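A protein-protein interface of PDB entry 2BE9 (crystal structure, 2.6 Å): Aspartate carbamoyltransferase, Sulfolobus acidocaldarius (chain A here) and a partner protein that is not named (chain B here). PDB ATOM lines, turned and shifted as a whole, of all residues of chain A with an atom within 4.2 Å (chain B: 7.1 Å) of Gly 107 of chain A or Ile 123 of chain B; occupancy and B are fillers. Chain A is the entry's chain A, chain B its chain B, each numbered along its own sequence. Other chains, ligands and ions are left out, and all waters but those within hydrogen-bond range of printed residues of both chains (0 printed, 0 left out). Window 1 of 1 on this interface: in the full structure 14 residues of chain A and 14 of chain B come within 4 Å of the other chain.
Of the printed residues of chain B, Arg 110 of chain A touches Glu 147 and Tyr 148.
Cys 117 of chain B touches none of the printed residues of chain A.
Printed residues of chain A within 4 Å of Asn 119 of chain B: Asp 106 (2.6 Å).
Printed residues of chain A within 4 Å of Cys 122 of chain B: Asp 106.
Of the printed residues of chain A, Ile 123 of chain B touches Leu 85, Asp 106 and Gly 107.
Of the printed residues of chain A, Cys 149 of chain B touches Asp 106 (3.4 Å).
The side-chain carboxylate (OD1) of Asp 127 of chain B is in hydrogen-bond range of the backbone NH (N) of Ala 130 of chain B.
ND2 of Asn 119 of chain B sits close to SG of Cys 149 of chain B, at 3.5 Å.
The backbone carbonyl oxygen (O) of Asn 119 of chain B sits at hydrogen-bond distance from the side-chain hydroxyl (OG) of Ser 125 of chain B, 2.9 Å away.
The backbone NH of Gly 107 of chain A is in hydrogen-bond range of the side-chain carboxylate of Asp 125 of chain A (3.0 Å).
O of Pro 120 of chain B sits at hydrogen-bond distance from ND2 of Asn 126 of chain B, 2.9 Å away.
N of Asn 119 of chain B sits close to SG of Cys 117 of chain B, at 3.6 Å.
The backbone NH of Asp 106 of chain A sits at hydrogen-bond distance from the backbone carbonyl oxygen of Tyr 121 of chain B (2.9 Å).
The guanidinium group of Arg 110 of chain A lies within salt-bridge range of the side-chain carboxylate of Glu 147 of chain B, 3.2 Å away.
OD2 of Asp 106 of chain A sits at hydrogen-bond distance from ND2 of Asn 119 of chain B (2.6 Å).
The side-chain hydroxyl (OH) of Tyr 105 of chain A sits at hydrogen-bond distance from the side-chain amide oxygen (OD1) of Asn 126 of chain B.
The backbone carbonyl oxygen (O) of Asp 106 of chain A is in hydrogen-bond range of the backbone NH (N) of Ile 123 of chain B, 2.8 Å away.
N of Leu 85 of chain A sits at hydrogen-bond distance from OD2 of Asp 127 of chain B (3.1 Å).
Hydrophobic or aromatic side chains of chain B within 4 Å of the printed part of chain A: Tyr 121, Ile 123, Ala 130 and Tyr 148.
Printed residues of chain A that touch a printed residue of chain B: Leu 85, Tyr 105, Asp 106, Gly 107, Arg 110 and Phe 111.
Among the printed residues, 17 pairs touch across the chains.
Among the printed residues, Asp or Glu carboxylates within 4 Å of a Lys or Arg side-chain nitrogen of the other chain: Arg 110 of chain A with Glu 147 of chain B (3.2 Å).
Ile 123 of chain B touches Leu 85 of chain A (CD1 to CD1, 3.8 Å).
CA of Tyr 105 of chain A touches O of Tyr 121 of chain B (3.1 Å).
Asp 106 of chain A touches Cys 122 of chain B (O to CA, 3.7 Å).
Cys 149 of chain B touches Asp 106 of chain A.
Gly 107 of chain A touches Ile 123 of chain B (O to CG2, 3.3 Å).
CD1 of Tyr 148 of chain B touches CD of Arg 110 of chain A, at 3.9 Å.
CE1 of Phe 111 of chain A touches OD2 of Asp 127 of chain B, at 3.3 Å.
CE2 of Phe 111 of chain A touches O of Glu 129 of chain B (3.4 Å).
Phe 111 of chain A touches Ala 130 of chain B (CE2 to CA, 3.6 Å).
Phe 111 of chain A touches Tyr 148 of chain B (CB to CE1, 3.7 Å).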
ATOM      1  N   LEU A  85      25.163 -21.740  13.423  1.00  0.00           N
ATOM      2  CA  LEU A  85      25.383 -22.599  12.256  1.00  0.00           C
ATOM      3  C   LEU A  85      25.976 -21.786  11.100  1.00  0.00           C
ATOM      4  O   LEU A  85      26.966 -22.207  10.476  1.00  0.00           O
ATOM      5  CB  LEU A  85      24.111 -23.291  11.782  1.00  0.00           C
ATOM      6  CG  LEU A  85      24.172 -24.663  11.077  1.00  0.00           C
ATOM      7  CD1 LEU A  85      23.096 -24.799   9.996  1.00  0.00           C
ATOM      8  CD2 LEU A  85      25.527 -25.087  10.508  1.00  0.00           C
ATOM      9  N   TYR A 105      18.872 -30.188  13.717  1.00  0.00           N
ATOM     10  CA  TYR A 105      17.785 -29.254  13.391  1.00  0.00           C
ATOM     11  C   TYR A 105      17.254 -29.431  11.970  1.00  0.00           C
ATOM     12  O   TYR A 105      18.031 -29.491  11.025  1.00  0.00           O
ATOM     13  CB  TYR A 105      18.209 -27.803  13.655  1.00  0.00           C
ATOM     14  CG  TYR A 105      18.488 -27.487  15.122  1.00  0.00           C
ATOM     15  CD1 TYR A 105      17.668 -27.998  16.150  1.00  0.00           C
ATOM     16  CD2 TYR A 105      19.559 -26.672  15.486  1.00  0.00           C
ATOM     17  CE1 TYR A 105      17.930 -27.725  17.493  1.00  0.00           C
ATOM     18  CE2 TYR A 105      19.824 -26.380  16.830  1.00  0.00           C
ATOM     19  CZ  TYR A 105      19.006 -26.905  17.826  1.00  0.00           C
ATOM     20  OH  TYR A 105      19.274 -26.611  19.156  1.00  0.00           O
ATOM     21  N   ASP A 106      15.931 -29.525  11.823  1.00  0.00           N
ATOM     22  CA  ASP A 106      15.319 -29.639  10.494  1.00  0.00           C
ATOM     23  C   ASP A 106      15.620 -28.395   9.676  1.00  0.00           C
ATOM     24  O   ASP A 106      15.480 -27.278  10.165  1.00  0.00           O
ATOM     25  CB  ASP A 106      13.799 -29.793  10.558  1.00  0.00           C
ATOM     26  CG  ASP A 106      13.346 -30.896  11.475  1.00  0.00           C
ATOM     27  OD1 ASP A 106      13.775 -32.046  11.335  1.00  0.00           O
ATOM     28  OD2 ASP A 106      12.502 -30.606  12.333  1.00  0.00           O
ATOM     29  N   GLY A 107      16.042 -28.610   8.433  1.00  0.00           N
ATOM     30  CA  GLY A 107      16.297 -27.536   7.498  1.00  0.00           C
ATOM     31  C   GLY A 107      17.712 -27.018   7.620  1.00  0.00           C
ATOM     32  O   GLY A 107      18.045 -25.987   7.013  1.00  0.00           O
ATOM     33  N   ALA A 108      18.559 -27.710   8.389  1.00  0.00           N
ATOM     34  CA  ALA A 108      19.894 -27.177   8.646  1.00  0.00           C
ATOM     35  C   ALA A 108      20.720 -27.169   7.366  1.00  0.00           C
ATOM     36  O   ALA A 108      21.465 -26.213   7.091  1.00  0.00           O
ATOM     37  CB  ALA A 108      20.579 -27.938   9.731  1.00  0.00           C
ATOM     38  N   SER A 109      20.541 -28.214   6.561  1.00  0.00           N
ATOM     39  CA  SER A 109      21.280 -28.342   5.314  1.00  0.00           C
ATOM     40  C   SER A 109      20.834 -27.325   4.286  1.00  0.00           C
ATOM     41  O   SER A 109      21.683 -26.749   3.580  1.00  0.00           O
ATOM     42  CB  SER A 109      21.157 -29.749   4.743  1.00  0.00           C
ATOM     43  OG  SER A 109      22.142 -30.571   5.333  1.00  0.00           O
ATOM     44  N   ARG A 110      19.515 -27.109   4.204  1.00  0.00           N
ATOM     45  CA  ARG A 110      18.974 -26.093   3.312  1.00  0.00           C
ATOM     46  C   ARG A 110      19.561 -24.701   3.650  1.00  0.00           C
ATOM     47  O   ARG A 110      20.058 -24.001   2.770  1.00  0.00           O
ATOM     48  CB  ARG A 110      17.443 -26.071   3.334  1.00  0.00           C
ATOM     49  CG  ARG A 110      16.839 -25.170   2.242  1.00  0.00           C
ATOM     50  CD  ARG A 110      15.348 -25.021   2.426  1.00  0.00           C
ATOM     51  NE  ARG A 110      14.639 -24.791   1.166  1.00  0.00           N
ATOM     52  CZ  ARG A 110      14.245 -23.598   0.723  1.00  0.00           C
ATOM     53  NH1 ARG A 110      14.485 -22.494   1.427  1.00  0.00           N
ATOM     54  NH2 ARG A 110      13.611 -23.505  -0.435  1.00  0.00           N
ATOM     55  N   PHE A 111      19.538 -24.340   4.932  1.00  0.00           N
ATOM     56  CA  PHE A 111      20.080 -23.069   5.370  1.00  0.00           C
ATOM     57  C   PHE A 111      21.583 -22.998   5.089  1.00  0.00           C
ATOM     58  O   PHE A 111      22.077 -21.997   4.558  1.00  0.00           O
ATOM     59  CB  PHE A 111      19.752 -22.798   6.855  1.00  0.00           C
ATOM     60  CG  PHE A 111      20.380 -21.546   7.395  1.00  0.00           C
ATOM     61  CD1 PHE A 111      21.372 -21.616   8.376  1.00  0.00           C
ATOM     62  CD2 PHE A 111      20.009 -20.288   6.907  1.00  0.00           C
ATOM     63  CE1 PHE A 111      21.983 -20.449   8.875  1.00  0.00           C
ATOM     64  CE2 PHE A 111      20.607 -19.108   7.403  1.00  0.00           C
ATOM     65  CZ  PHE A 111      21.596 -19.194   8.390  1.00  0.00           C
ATOM     66  N   ASP A 125      19.184 -34.158   8.434  1.00  0.00           N
ATOM     67  CA  ASP A 125      18.813 -32.920   9.100  1.00  0.00           C
ATOM     68  C   ASP A 125      17.556 -33.154   9.963  1.00  0.00           C
ATOM     69  O   ASP A 125      16.443 -33.326   9.435  1.00  0.00           O
ATOM     70  CB  ASP A 125      18.630 -31.803   8.061  1.00  0.00           C
ATOM     71  CG  ASP A 125      17.443 -32.042   7.127  1.00  0.00           C
ATOM     72  OD1 ASP A 125      17.219 -33.207   6.702  1.00  0.00           O
ATOM     73  OD2 ASP A 125      16.723 -31.053   6.834  1.00  0.00           O
ATOM     74  N   CYS B 117       8.385 -20.313  13.099  1.00  0.00           N
ATOM     75  CA  CYS B 117       8.029 -21.707  12.899  1.00  0.00           C
ATOM     76  C   CYS B 117       7.745 -22.366  14.247  1.00  0.00           C
ATOM     77  O   CYS B 117       8.577 -22.311  15.166  1.00  0.00           O
ATOM     78  CB  CYS B 117       9.131 -22.450  12.132  1.00  0.00           C
ATOM     79  SG  CYS B 117       8.747 -24.177  11.667  1.00  0.00           S
ATOM     80  N   ASN B 119       7.818 -25.419  14.957  1.00  0.00           N
ATOM     81  CA  ASN B 119       8.737 -26.538  15.212  1.00  0.00           C
ATOM     82  C   ASN B 119       9.984 -26.107  16.007  1.00  0.00           C
ATOM     83  O   ASN B 119      10.840 -25.413  15.483  1.00  0.00           O
ATOM     84  CB  ASN B 119       9.102 -27.267  13.906  1.00  0.00           C
ATOM     85  CG  ASN B 119      10.233 -28.288  14.088  1.00  0.00           C
ATOM     86  OD1 ASN B 119      10.510 -28.750  15.200  1.00  0.00           O
ATOM     87  ND2 ASN B 119      10.894 -28.640  12.983  1.00  0.00           N
ATOM     88  N   PRO B 120      10.090 -26.532  17.285  1.00  0.00           N
ATOM     89  CA  PRO B 120      11.239 -26.100  18.079  1.00  0.00           C
ATOM     90  C   PRO B 120      12.569 -26.596  17.502  1.00  0.00           C
ATOM     91  O   PRO B 120      13.615 -26.041  17.823  1.00  0.00           O
ATOM     92  CB  PRO B 120      10.974 -26.734  19.447  1.00  0.00           C
ATOM     93  CG  PRO B 120      10.085 -27.895  19.164  1.00  0.00           C
ATOM     94  CD  PRO B 120       9.204 -27.429  18.063  1.00  0.00           C
ATOM     95  N   TYR B 121      12.511 -27.615  16.647  1.00  0.00           N
ATOM     96  CA  TYR B 121      13.699 -28.207  16.024  1.00  0.00           C
ATOM     97  C   TYR B 121      14.024 -27.614  14.670  1.00  0.00           C
ATOM     98  O   TYR B 121      15.045 -27.949  14.091  1.00  0.00           O
ATOM     99  CB  TYR B 121      13.548 -29.723  15.909  1.00  0.00           C
ATOM    100  CG  TYR B 121      13.540 -30.353  17.267  1.00  0.00           C
ATOM    101  CD1 TYR B 121      12.340 -30.706  17.886  1.00  0.00           C
ATOM    102  CD2 TYR B 121      14.736 -30.530  17.968  1.00  0.00           C
ATOM    103  CE1 TYR B 121      12.334 -31.246  19.147  1.00  0.00           C
ATOM    104  CE2 TYR B 121      14.742 -31.067  19.226  1.00  0.00           C
ATOM    105  CZ  TYR B 121      13.540 -31.420  19.810  1.00  0.00           C
ATOM    106  OH  TYR B 121      13.558 -31.959  21.062  1.00  0.00           O
ATOM    107  N   CYS B 122      13.163 -26.728  14.175  1.00  0.00           N
ATOM    108  CA  CYS B 122      13.429 -26.025  12.937  1.00  0.00           C
ATOM    109  C   CYS B 122      14.659 -25.175  13.113  1.00  0.00           C
ATOM    110  O   CYS B 122      14.803 -24.489  14.127  1.00  0.00           O
ATOM    111  CB  CYS B 122      12.262 -25.137  12.546  1.00  0.00           C
ATOM    112  SG  CYS B 122      12.428 -24.461  10.881  1.00  0.00           S
ATOM    113  N   ILE B 123      15.545 -25.232  12.121  1.00  0.00           N
ATOM    114  CA  ILE B 123      16.722 -24.391  12.093  1.00  0.00           C
ATOM    115  C   ILE B 123      16.386 -22.887  12.278  1.00  0.00           C
ATOM    116  O   ILE B 123      17.128 -22.155  12.959  1.00  0.00           O
ATOM    117  CB  ILE B 123      17.540 -24.630  10.800  1.00  0.00           C
ATOM    118  CG1 ILE B 123      18.857 -23.852  10.840  1.00  0.00           C
ATOM    119  CG2 ILE B 123      16.705 -24.329   9.549  1.00  0.00           C
ATOM    120  CD1 ILE B 123      19.828 -24.361  11.871  1.00  0.00           C
ATOM    121  N   THR B 124      15.264 -22.445  11.699  1.00  0.00           N
ATOM    122  CA  THR B 124      14.794 -21.070  11.863  1.00  0.00           C
ATOM    123  C   THR B 124      14.408 -20.709  13.311  1.00  0.00           C
ATOM    124  O   THR B 124      14.280 -19.522  13.638  1.00  0.00           O
ATOM    125  CB  THR B 124      13.633 -20.722  10.886  1.00  0.00           C
ATOM    126  OG1 THR B 124      12.452 -21.433  11.255  1.00  0.00           O
ATOM    127  CG2 THR B 124      14.003 -21.091   9.433  1.00  0.00           C
ATOM    128  N   SER B 125      14.235 -21.723  14.166  1.00  0.00           N
ATOM    129  CA  SER B 125      13.910 -21.516  15.594  1.00  0.00           C
ATOM    130  C   SER B 125      15.170 -21.519  16.459  1.00  0.00           C
ATOM    131  O   SER B 125      15.079 -21.498  17.685  1.00  0.00           O
ATOM    132  CB  SER B 125      13.002 -22.627  16.134  1.00  0.00           C
ATOM    133  OG  SER B 125      11.768 -22.695  15.461  1.00  0.00           O
ATOM    134  N   ASN B 126      16.340 -21.587  15.834  1.00  0.00           N
ATOM    135  CA  ASN B 126      17.569 -21.757  16.598  1.00  0.00           C
ATOM    136  C   ASN B 126      18.722 -20.860  16.139  1.00  0.00           C
ATOM    137  O   ASN B 126      19.483 -20.330  16.968  1.00  0.00           O
ATOM    138  CB  ASN B 126      17.995 -23.229  16.628  1.00  0.00           C
ATOM    139  CG  ASN B 126      17.002 -24.108  17.399  1.00  0.00           C
ATOM    140  OD1 ASN B 126      17.231 -24.413  18.566  1.00  0.00           O
ATOM    141  ND2 ASN B 126      15.894 -24.507  16.750  1.00  0.00           N
ATOM    142  N   ASP B 127      18.848 -20.673  14.832  1.00  0.00           N
ATOM    143  CA  ASP B 127      19.906 -19.840  14.325  1.00  0.00           C
ATOM    144  C   ASP B 127      19.334 -18.448  14.060  1.00  0.00           C
ATOM    145  O   ASP B 127      18.433 -18.307  13.236  1.00  0.00           O
ATOM    146  CB  ASP B 127      20.516 -20.499  13.073  1.00  0.00           C
ATOM    147  CG  ASP B 127      21.712 -19.747  12.525  1.00  0.00           C
ATOM    148  OD1 ASP B 127      21.674 -18.493  12.461  1.00  0.00           O
ATOM    149  OD2 ASP B 127      22.695 -20.416  12.143  1.00  0.00           O
ATOM    150  N   VAL B 128      19.846 -17.436  14.769  1.00  0.00           N
ATOM    151  CA  VAL B 128      19.412 -16.037  14.585  1.00  0.00           C
ATOM    152  C   VAL B 128      19.424 -15.561  13.143  1.00  0.00           C
ATOM    153  O   VAL B 128      18.597 -14.744  12.767  1.00  0.00           O
ATOM    154  CB  VAL B 128      20.234 -14.998  15.411  1.00  0.00           C
ATOM    155  CG1 VAL B 128      19.759 -14.975  16.848  1.00  0.00           C
ATOM    156  CG2 VAL B 128      21.763 -15.247  15.315  1.00  0.00           C
ATOM    157  N   GLU B 129      20.376 -16.056  12.351  1.00  0.00           N
ATOM    158  CA  GLU B 129      20.488 -15.668  10.945  1.00  0.00           C
ATOM    159  C   GLU B 129      19.601 -16.523  10.063  1.00  0.00           C
ATOM    160  O   GLU B 129      19.443 -16.239   8.882  1.00  0.00           O
ATOM    161  CB  GLU B 129      21.927 -15.756  10.450  1.00  0.00           C
ATOM    162  CG  GLU B 129      22.851 -14.680  10.969  1.00  0.00           C
ATOM    163  CD  GLU B 129      24.188 -14.740  10.286  1.00  0.00           C
ATOM    164  OE1 GLU B 129      24.237 -14.354   9.111  1.00  0.00           O
ATOM    165  OE2 GLU B 129      25.185 -15.188  10.895  1.00  0.00           O
ATOM    166  N   ALA B 130      19.020 -17.567  10.635  1.00  0.00           N
ATOM    167  CA  ALA B 130      18.136 -18.412   9.880  1.00  0.00           C
ATOM    168  C   ALA B 130      16.715 -17.851   9.976  1.00  0.00           C
ATOM    169  O   ALA B 130      15.951 -18.187  10.875  1.00  0.00           O
ATOM    170  CB  ALA B 130      18.219 -19.847  10.384  1.00  0.00           C
ATOM    171  N   ILE B 131      16.369 -16.990   9.036  1.00  0.00           N
ATOM    172  CA  ILE B 131      15.119 -16.257   9.091  1.00  0.00           C
ATOM    173  C   ILE B 131      13.906 -17.090   8.645  1.00  0.00           C
ATOM    174  O   ILE B 131      13.868 -17.619   7.524  1.00  0.00           O
ATOM    175  CB  ILE B 131      15.243 -14.940   8.334  1.00  0.00           C
ATOM    176  CG1 ILE B 131      16.196 -14.019   9.119  1.00  0.00           C
ATOM    177  CG2 ILE B 131      13.874 -14.284   8.157  1.00  0.00           C
ATOM    178  CD1 ILE B 131      16.746 -12.840   8.313  1.00  0.00           C
ATOM    179  N   CYS B 146       6.450 -24.087   6.142  1.00  0.00           N
ATOM    180  CA  CYS B 146       7.836 -23.683   6.441  1.00  0.00           C
ATOM    181  C   CYS B 146       8.770 -24.261   5.389  1.00  0.00           C
ATOM    182  O   CYS B 146       8.746 -25.470   5.138  1.00  0.00           O
ATOM    183  CB  CYS B 146       8.242 -24.184   7.827  1.00  0.00           C
ATOM    184  SG  CYS B 146       9.970 -24.032   8.237  1.00  0.00           S
ATOM    185  N   GLU B 147       9.589 -23.410   4.775  1.00  0.00           N
ATOM    186  CA  GLU B 147      10.449 -23.850   3.665  1.00  0.00           C
ATOM    187  C   GLU B 147      11.646 -24.680   4.096  1.00  0.00           C
ATOM    188  O   GLU B 147      12.317 -25.279   3.254  1.00  0.00           O
ATOM    189  CB  GLU B 147      10.955 -22.661   2.860  1.00  0.00           C
ATOM    190  CG  GLU B 147       9.864 -21.901   2.092  1.00  0.00           C
ATOM    191  CD  GLU B 147      10.464 -20.926   1.100  1.00  0.00           C
ATOM    192  OE1 GLU B 147      11.716 -20.941   0.939  1.00  0.00           O
ATOM    193  OE2 GLU B 147       9.688 -20.155   0.492  1.00  0.00           O
ATOM    194  N   TYR B 148      11.906 -24.713   5.401  1.00  0.00           N
ATOM    195  CA  TYR B 148      13.047 -25.446   5.921  1.00  0.00           C
ATOM    196  C   TYR B 148      12.663 -26.830   6.414  1.00  0.00           C
ATOM    197  O   TYR B 148      13.329 -27.810   6.096  1.00  0.00           O
ATOM    198  CB  TYR B 148      13.729 -24.642   7.028  1.00  0.00           C
ATOM    199  CG  TYR B 148      14.397 -23.420   6.476  1.00  0.00           C
ATOM    200  CD1 TYR B 148      15.728 -23.476   6.016  1.00  0.00           C
ATOM    201  CD2 TYR B 148      13.701 -22.213   6.366  1.00  0.00           C
ATOM    202  CE1 TYR B 148      16.357 -22.356   5.482  1.00  0.00           C
ATOM    203  CE2 TYR B 148      14.318 -21.089   5.825  1.00  0.00           C
ATOM    204  CZ  TYR B 148      15.647 -21.167   5.382  1.00  0.00           C
ATOM    205  OH  TYR B 148      16.257 -20.059   4.848  1.00  0.00           O
ATOM    206  N   CYS B 149      11.572 -26.911   7.172  1.00  0.00           N
ATOM    207  CA  CYS B 149      11.197 -28.152   7.842  1.00  0.00           C
ATOM    208  C   CYS B 149       9.840 -28.702   7.398  1.00  0.00           C
ATOM    209  O   CYS B 149       9.456 -29.785   7.823  1.00  0.00           O
ATOM    210  CB  CYS B 149      11.220 -27.966   9.363  1.00  0.00           C
ATOM    211  SG  CYS B 149       9.797 -27.107  10.034  1.00  0.00           S
